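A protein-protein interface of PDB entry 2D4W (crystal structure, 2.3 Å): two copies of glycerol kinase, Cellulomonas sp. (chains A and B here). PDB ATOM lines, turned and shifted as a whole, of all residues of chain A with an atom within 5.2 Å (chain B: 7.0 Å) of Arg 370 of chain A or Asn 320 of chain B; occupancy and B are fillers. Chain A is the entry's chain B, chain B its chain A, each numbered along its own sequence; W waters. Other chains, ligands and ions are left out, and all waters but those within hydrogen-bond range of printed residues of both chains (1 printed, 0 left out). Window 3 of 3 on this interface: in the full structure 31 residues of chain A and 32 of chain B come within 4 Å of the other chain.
No position is printed for both chains.
Of the 12 pairs that touch across the chains among the printed residues, none has its exchanged pair printed and touching as well.
O of Asn 320 of chain B is in hydrogen-bond range of N of Arg 374 of chain A, at 2.8 Å.
The backbone carbonyl oxygen of Leu 368 of chain A lies close to the backbone carbonyl oxygen of Ala 361 of chain B (3.5 Å).
The indole nitrogen (NE1) of Trp 316 of chain B lies within hydrogen-bond range of the backbone carbonyl oxygen (O) of Thr 369 of chain A (3.3 Å).
The backbone carbonyl oxygen (O) of Val 372 of chain A sits at hydrogen-bond distance from the indole nitrogen (NE1) of Trp 316 of chain B, at 3.2 Å.
O of Val 372 of chain A lies within hydrogen-bond range of ND2 of Asn 320 of chain B (3.0 Å).
O of Arg 370 of chain A lies within hydrogen-bond range of ND2 of Asn 320 of chain B.
Printed residues of chain B that touch a printed residue of chain A: Trp 316, Asn 320, Leu 321 and Ala 361.
Along chain B the printed residues that touch a printed residue of chain A span positions 316 to 361.
Among the printed residues, 12 pairs touch across the chains.
Among the printed residues, no Asp or Glu carboxylate lies within 4 Å of a Lys or Arg side-chain nitrogen of the other chain.
O of Trp 316 of chain B is in hydrogen-bond range of N of Leu 321 of chain B.
Water W1 lies within hydrogen-bond range of O of Ala 361 of chain B (2.8 Å) and N of Arg 370 of chain A (3.0 Å).
Arg 370 of chain A touches two residues of chain B.
Asn 320 of chain B touches just these residues of chain A: Arg 370 (3.2 Å), Val 372 (3.0 Å), Asn 373 (3.4 Å) and Arg 374 (2.8 Å).
Printed residues of chain A within 4 Å of Trp 316 of chain B: Leu 368, Thr 369, Arg 370 and Val 372.
Printed residues of chain A within 4 Å of Ala 361 of chain B: Leu 368 (3.5 Å) and Thr 369 (3.4 Å).
Of the printed residues of chain B, Arg 374 of chain A touches Asn 320 (2.8 Å) and Leu 321 (3.8 Å).
Printed residues of chain B within 4 Å of Asn 373 of chain A: Asn 320 (3.4 Å) and Leu 321 (3.8 Å).
Asp 319 of chain B touches none of the printed residues of chain A.
The nearest residue of chain A that does not touch Asn 320 of chain B is Tyr 371 of chain A (4.2 Å).
Among the printed residues, pairs that only touch across the chains: Asn 373 of chain A with Asn 320 of chain B (3.4 Å), Thr 369 of chain A with Ala 361 of chain B (3.4 Å), Arg 370 of chain A with Trp 316 of chain B (3.6 Å), Arg 374 of chain A with Leu 321 of chain B (3.8 Å), Asn 373 of chain A with Leu 321 of chain B (3.8 Å) and Leu 368 of chain A with Trp 316 of chain B (3.9 Å).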
ATOM      1  N   LEU A 368      20.913  11.649 -21.389  1.00  0.00           N
ATOM      2  CA  LEU A 368      20.950  10.206 -21.604  1.00  0.00           C
ATOM      3  C   LEU A 368      21.664   9.518 -20.467  1.00  0.00           C
ATOM      4  O   LEU A 368      22.751   9.937 -20.074  1.00  0.00           O
ATOM      5  CB  LEU A 368      21.669   9.842 -22.933  1.00  0.00           C
ATOM      6  CG  LEU A 368      20.963  10.402 -24.186  1.00  0.00           C
ATOM      7  CD1 LEU A 368      21.650   9.950 -25.496  1.00  0.00           C
ATOM      8  CD2 LEU A 368      19.518   9.967 -24.240  1.00  0.00           C
ATOM      9  N   THR A 369      21.064   8.458 -19.952  1.00  0.00           N
ATOM     10  CA  THR A 369      21.684   7.661 -18.908  1.00  0.00           C
ATOM     11  C   THR A 369      21.467   6.191 -19.210  1.00  0.00           C
ATOM     12  O   THR A 369      20.725   5.816 -20.126  1.00  0.00           O
ATOM     13  CB  THR A 369      21.097   7.933 -17.496  1.00  0.00           C
ATOM     14  OG1 THR A 369      19.661   7.760 -17.524  1.00  0.00           O
ATOM     15  CG2 THR A 369      21.314   9.349 -17.058  1.00  0.00           C
ATOM     16  N   ARG A 370      22.108   5.361 -18.414  1.00  0.00           N
ATOM     17  CA  ARG A 370      22.023   3.928 -18.611  1.00  0.00           C
ATOM     18  C   ARG A 370      20.577   3.394 -18.595  1.00  0.00           C
ATOM     19  O   ARG A 370      20.314   2.368 -19.148  1.00  0.00           O
ATOM     20  CB  ARG A 370      22.793   3.238 -17.503  1.00  0.00           C
ATOM     21  CG  ARG A 370      23.049   1.752 -17.744  1.00  0.00           C
ATOM     22  CD  ARG A 370      23.428   0.998 -16.472  1.00  0.00           C
ATOM     23  NE  ARG A 370      23.788   1.919 -15.386  1.00  0.00           N
ATOM     24  CZ  ARG A 370      23.356   1.803 -14.123  1.00  0.00           C
ATOM     25  NH1 ARG A 370      22.546   0.803 -13.784  1.00  0.00           N
ATOM     26  NH2 ARG A 370      23.727   2.677 -13.187  1.00  0.00           N
ATOM     27  N   TYR A 371      19.620   4.077 -17.979  1.00  0.00           N
ATOM     28  CA  TYR A 371      18.305   3.468 -17.866  1.00  0.00           C
ATOM     29  C   TYR A 371      17.268   3.936 -18.863  1.00  0.00           C
ATOM     30  O   TYR A 371      16.177   3.359 -18.954  1.00  0.00           O
ATOM     31  CB  TYR A 371      17.779   3.608 -16.449  1.00  0.00           C
ATOM     32  CG  TYR A 371      18.505   2.642 -15.520  1.00  0.00           C
ATOM     33  CD1 TYR A 371      19.265   3.116 -14.445  1.00  0.00           C
ATOM     34  CD2 TYR A 371      18.480   1.272 -15.770  1.00  0.00           C
ATOM     35  CE1 TYR A 371      19.960   2.236 -13.600  1.00  0.00           C
ATOM     36  CE2 TYR A 371      19.174   0.355 -14.914  1.00  0.00           C
ATOM     37  CZ  TYR A 371      19.897   0.861 -13.834  1.00  0.00           C
ATOM     38  OH  TYR A 371      20.568  -0.025 -12.982  1.00  0.00           O
ATOM     39  N   VAL A 372      17.625   4.994 -19.575  1.00  0.00           N
ATOM     40  CA  VAL A 372      16.814   5.513 -20.649  1.00  0.00           C
ATOM     41  C   VAL A 372      16.820   4.455 -21.728  1.00  0.00           C
ATOM     42  O   VAL A 372      17.868   3.851 -22.028  1.00  0.00           O
ATOM     43  CB  VAL A 372      17.432   6.827 -21.220  1.00  0.00           C
ATOM     44  CG1 VAL A 372      16.804   7.247 -22.552  1.00  0.00           C
ATOM     45  CG2 VAL A 372      17.308   7.960 -20.224  1.00  0.00           C
ATOM     46  N   ASN A 373      15.632   4.195 -22.265  1.00  0.00           N
ATOM     47  CA  ASN A 373      15.468   3.240 -23.328  1.00  0.00           C
ATOM     48  C   ASN A 373      14.612   3.913 -24.403  1.00  0.00           C
ATOM     49  O   ASN A 373      14.314   5.105 -24.299  1.00  0.00           O
ATOM     50  CB  ASN A 373      14.889   1.903 -22.808  1.00  0.00           C
ATOM     51  CG  ASN A 373      13.526   2.052 -22.170  1.00  0.00           C
ATOM     52  OD1 ASN A 373      12.638   2.754 -22.700  1.00  0.00           O
ATOM     53  ND2 ASN A 373      13.339   1.412 -21.017  1.00  0.00           N
ATOM     54  N   ARG A 374      14.268   3.185 -25.457  1.00  0.00           N
ATOM     55  CA  ARG A 374      13.526   3.794 -26.580  1.00  0.00           C
ATOM     56  C   ARG A 374      12.121   4.217 -26.198  1.00  0.00           C
ATOM     57  O   ARG A 374      11.451   4.933 -26.932  1.00  0.00           O
ATOM     58  CB  ARG A 374      13.492   2.870 -27.810  1.00  0.00           C
ATOM     59  CG  ARG A 374      12.584   1.653 -27.622  1.00  0.00           C
ATOM     60  CD  ARG A 374      12.368   0.884 -28.920  1.00  0.00           C
ATOM     61  NE  ARG A 374      11.437  -0.241 -28.791  1.00  0.00           N
ATOM     62  CZ  ARG A 374      11.031  -0.967 -29.823  1.00  0.00           C
ATOM     63  NH1 ARG A 374      11.476  -0.681 -31.039  1.00  0.00           N
ATOM     64  NH2 ARG A 374      10.167  -1.964 -29.653  1.00  0.00           N
ATOM     65  N   VAL B 314      27.870   1.406 -27.541  1.00  0.00           N
ATOM     66  CA  VAL B 314      27.252   0.726 -28.643  1.00  0.00           C
ATOM     67  C   VAL B 314      26.288  -0.349 -28.120  1.00  0.00           C
ATOM     68  O   VAL B 314      25.233  -0.573 -28.709  1.00  0.00           O
ATOM     69  CB  VAL B 314      28.338   0.035 -29.561  1.00  0.00           C
ATOM     70  CG1 VAL B 314      27.726  -1.057 -30.435  1.00  0.00           C
ATOM     71  CG2 VAL B 314      29.078   1.081 -30.430  1.00  0.00           C
ATOM     72  N   GLN B 315      26.663  -1.029 -27.050  1.00  0.00           N
ATOM     73  CA  GLN B 315      25.798  -2.061 -26.454  1.00  0.00           C
ATOM     74  C   GLN B 315      24.495  -1.471 -25.932  1.00  0.00           C
ATOM     75  O   GLN B 315      23.446  -2.084 -26.015  1.00  0.00           O
ATOM     76  CB  GLN B 315      26.515  -2.829 -25.326  1.00  0.00           C
ATOM     77  CG  GLN B 315      25.880  -4.201 -25.023  1.00  0.00           C
ATOM     78  CD  GLN B 315      25.802  -5.098 -26.287  1.00  0.00           C
ATOM     79  OE1 GLN B 315      24.736  -5.647 -26.627  1.00  0.00           O
ATOM     80  NE2 GLN B 315      26.932  -5.225 -26.985  1.00  0.00           N
ATOM     81  N   TRP B 316      24.566  -0.262 -25.408  1.00  0.00           N
ATOM     82  CA  TRP B 316      23.368   0.449 -24.963  1.00  0.00           C
ATOM     83  C   TRP B 316      22.505   0.874 -26.173  1.00  0.00           C
ATOM     84  O   TRP B 316      21.278   0.818 -26.143  1.00  0.00           O
ATOM     85  CB  TRP B 316      23.806   1.693 -24.166  1.00  0.00           C
ATOM     86  CG  TRP B 316      22.706   2.591 -23.714  1.00  0.00           C
ATOM     87  CD1 TRP B 316      21.910   2.433 -22.591  1.00  0.00           C
ATOM     88  CD2 TRP B 316      22.273   3.810 -24.338  1.00  0.00           C
ATOM     89  NE1 TRP B 316      21.021   3.479 -22.507  1.00  0.00           N
ATOM     90  CE2 TRP B 316      21.213   4.325 -23.570  1.00  0.00           C
ATOM     91  CE3 TRP B 316      22.654   4.497 -25.487  1.00  0.00           C
ATOM     92  CZ2 TRP B 316      20.571   5.516 -23.890  1.00  0.00           C
ATOM     93  CZ3 TRP B 316      22.035   5.656 -25.801  1.00  0.00           C
ATOM     94  CH2 TRP B 316      20.990   6.172 -25.006  1.00  0.00           C
ATOM     95  N   LEU B 317      23.143   1.324 -27.243  1.00  0.00           N
ATOM     96  CA  LEU B 317      22.355   1.730 -28.430  1.00  0.00           C
ATOM     97  C   LEU B 317      21.509   0.536 -28.924  1.00  0.00           C
ATOM     98  O   LEU B 317      20.380   0.687 -29.410  1.00  0.00           O
ATOM     99  CB  LEU B 317      23.291   2.225 -29.517  1.00  0.00           C
ATOM    100  CG  LEU B 317      24.006   3.542 -29.165  1.00  0.00           C
ATOM    101  CD1 LEU B 317      25.146   3.848 -30.145  1.00  0.00           C
ATOM    102  CD2 LEU B 317      22.968   4.673 -29.149  1.00  0.00           C
ATOM    103  N   ARG B 318      22.034  -0.666 -28.717  1.00  0.00           N
ATOM    104  CA  ARG B 318      21.361  -1.882 -29.200  1.00  0.00           C
ATOM    105  C   ARG B 318      20.258  -2.360 -28.255  1.00  0.00           C
ATOM    106  O   ARG B 318      19.093  -2.481 -28.624  1.00  0.00           O
ATOM    107  CB  ARG B 318      22.416  -3.000 -29.387  1.00  0.00           C
ATOM    108  CG  ARG B 318      22.029  -4.082 -30.372  1.00  0.00           C
ATOM    109  CD  ARG B 318      23.205  -4.989 -30.870  1.00  0.00           C
ATOM    110  NE  ARG B 318      24.543  -4.432 -30.640  1.00  0.00           N
ATOM    111  CZ  ARG B 318      25.472  -4.359 -31.575  1.00  0.00           C
ATOM    112  NH1 ARG B 318      25.234  -4.776 -32.812  1.00  0.00           N
ATOM    113  NH2 ARG B 318      26.654  -3.854 -31.291  1.00  0.00           N
ATOM    114  N   ASP B 319      20.642  -2.603 -27.009  1.00  0.00           N
ATOM    115  CA  ASP B 319      19.723  -3.171 -26.053  1.00  0.00           C
ATOM    116  C   ASP B 319      18.716  -2.140 -25.549  1.00  0.00           C
ATOM    117  O   ASP B 319      17.601  -2.515 -25.181  1.00  0.00           O
ATOM    118  CB  ASP B 319      20.482  -3.777 -24.857  1.00  0.00           C
ATOM    119  CG  ASP B 319      21.597  -4.734 -25.274  1.00  0.00           C
ATOM    120  OD1 ASP B 319      21.510  -5.377 -26.341  1.00  0.00           O
ATOM    121  OD2 ASP B 319      22.623  -4.912 -24.587  1.00  0.00           O
ATOM    122  N   ASN B 320      19.086  -0.859 -25.512  1.00  0.00           N
ATOM    123  CA  ASN B 320      18.136   0.132 -25.000  1.00  0.00           C
ATOM    124  C   ASN B 320      17.384   0.911 -26.073  1.00  0.00           C
ATOM    125  O   ASN B 320      16.196   1.192 -25.930  1.00  0.00           O
ATOM    126  CB  ASN B 320      18.778   1.079 -23.961  1.00  0.00           C
ATOM    127  CG  ASN B 320      19.011   0.394 -22.607  1.00  0.00           C
ATOM    128  OD1 ASN B 320      19.566  -0.689 -22.557  1.00  0.00           O
ATOM    129  ND2 ASN B 320      18.574   1.011 -21.530  1.00  0.00           N
ATOM    130  N   LEU B 321      18.062   1.283 -27.149  1.00  0.00           N
ATOM    131  CA  LEU B 321      17.358   2.021 -28.185  1.00  0.00           C
ATOM    132  C   LEU B 321      16.864   1.098 -29.345  1.00  0.00           C
ATOM    133  O   LEU B 321      16.083   1.521 -30.183  1.00  0.00           O
ATOM    134  CB  LEU B 321      18.197   3.189 -28.677  1.00  0.00           C
ATOM    135  CG  LEU B 321      18.677   4.261 -27.662  1.00  0.00           C
ATOM    136  CD1 LEU B 321      19.196   5.497 -28.362  1.00  0.00           C
ATOM    137  CD2 LEU B 321      17.607   4.691 -26.668  1.00  0.00           C
ATOM    138  N   GLY B 322      17.317  -0.153 -29.387  1.00  0.00           N
ATOM    139  CA  GLY B 322      16.917  -1.060 -30.444  1.00  0.00           C
ATOM    140  C   GLY B 322      17.622  -0.785 -31.759  1.00  0.00           C
ATOM    141  O   GLY B 322      17.129  -1.130 -32.814  1.00  0.00           O
ATOM    142  N   MET B 323      18.783  -0.140 -31.712  1.00  0.00           N
ATOM    143  CA  MET B 323      19.508   0.135 -32.942  1.00  0.00           C
ATOM    144  C   MET B 323      20.403  -1.006 -33.352  1.00  0.00           C
ATOM    145  O   MET B 323      20.770  -1.839 -32.534  1.00  0.00           O
ATOM    146  CB  MET B 323      20.340   1.404 -32.806  1.00  0.00           C
ATOM    147  CG  MET B 323      19.489   2.678 -32.872  1.00  0.00           C
ATOM    148  SD  MET B 323      20.438   4.183 -32.636  1.00  0.00           S
ATOM    149  CE  MET B 323      21.460   4.179 -34.149  1.00  0.00           C
ATOM    150  N   ALA B 348      28.521   9.147 -21.075  1.00  0.00           N
ATOM    151  CA  ALA B 348      28.324   9.364 -19.625  1.00  0.00           C
ATOM    152  C   ALA B 348      29.644   9.180 -18.856  1.00  0.00           C
ATOM    153  O   ALA B 348      30.321   8.212 -19.159  1.00  0.00           O
ATOM    154  CB  ALA B 348      27.276   8.357 -19.069  1.00  0.00           C
ATOM    155  N   PHE B 349      29.970  10.111 -17.941  1.00  0.00           N
ATOM    156  CA  PHE B 349      31.176  10.117 -17.173  1.00  0.00           C
ATOM    157  C   PHE B 349      32.372  10.480 -18.011  1.00  0.00           C
ATOM    158  O   PHE B 349      33.494  10.224 -17.597  1.00  0.00           O
ATOM    159  CB  PHE B 349      31.400   8.736 -16.553  1.00  0.00           C
ATOM    160  CG  PHE B 349      30.201   8.194 -15.818  1.00  0.00           C
ATOM    161  CD1 PHE B 349      29.500   7.112 -16.304  1.00  0.00           C
ATOM    162  CD2 PHE B 349      29.837   8.727 -14.587  1.00  0.00           C
ATOM    163  CE1 PHE B 349      28.416   6.596 -15.602  1.00  0.00           C
ATOM    164  CE2 PHE B 349      28.767   8.206 -13.842  1.00  0.00           C
ATOM    165  CZ  PHE B 349      28.033   7.145 -14.375  1.00  0.00           C
ATOM    166  N   ALA B 361      26.672  11.068 -14.690  1.00  0.00           N
ATOM    167  CA  ALA B 361      26.000   9.914 -15.289  1.00  0.00           C
ATOM    168  C   ALA B 361      25.181  10.307 -16.516  1.00  0.00           C
ATOM    169  O   ALA B 361      24.705   9.462 -17.249  1.00  0.00           O
ATOM    170  CB  ALA B 361      25.070   9.229 -14.256  1.00  0.00           C
HETATM  171  O   HOH W   1      24.442   6.651 -17.075  1.00  0.00           O
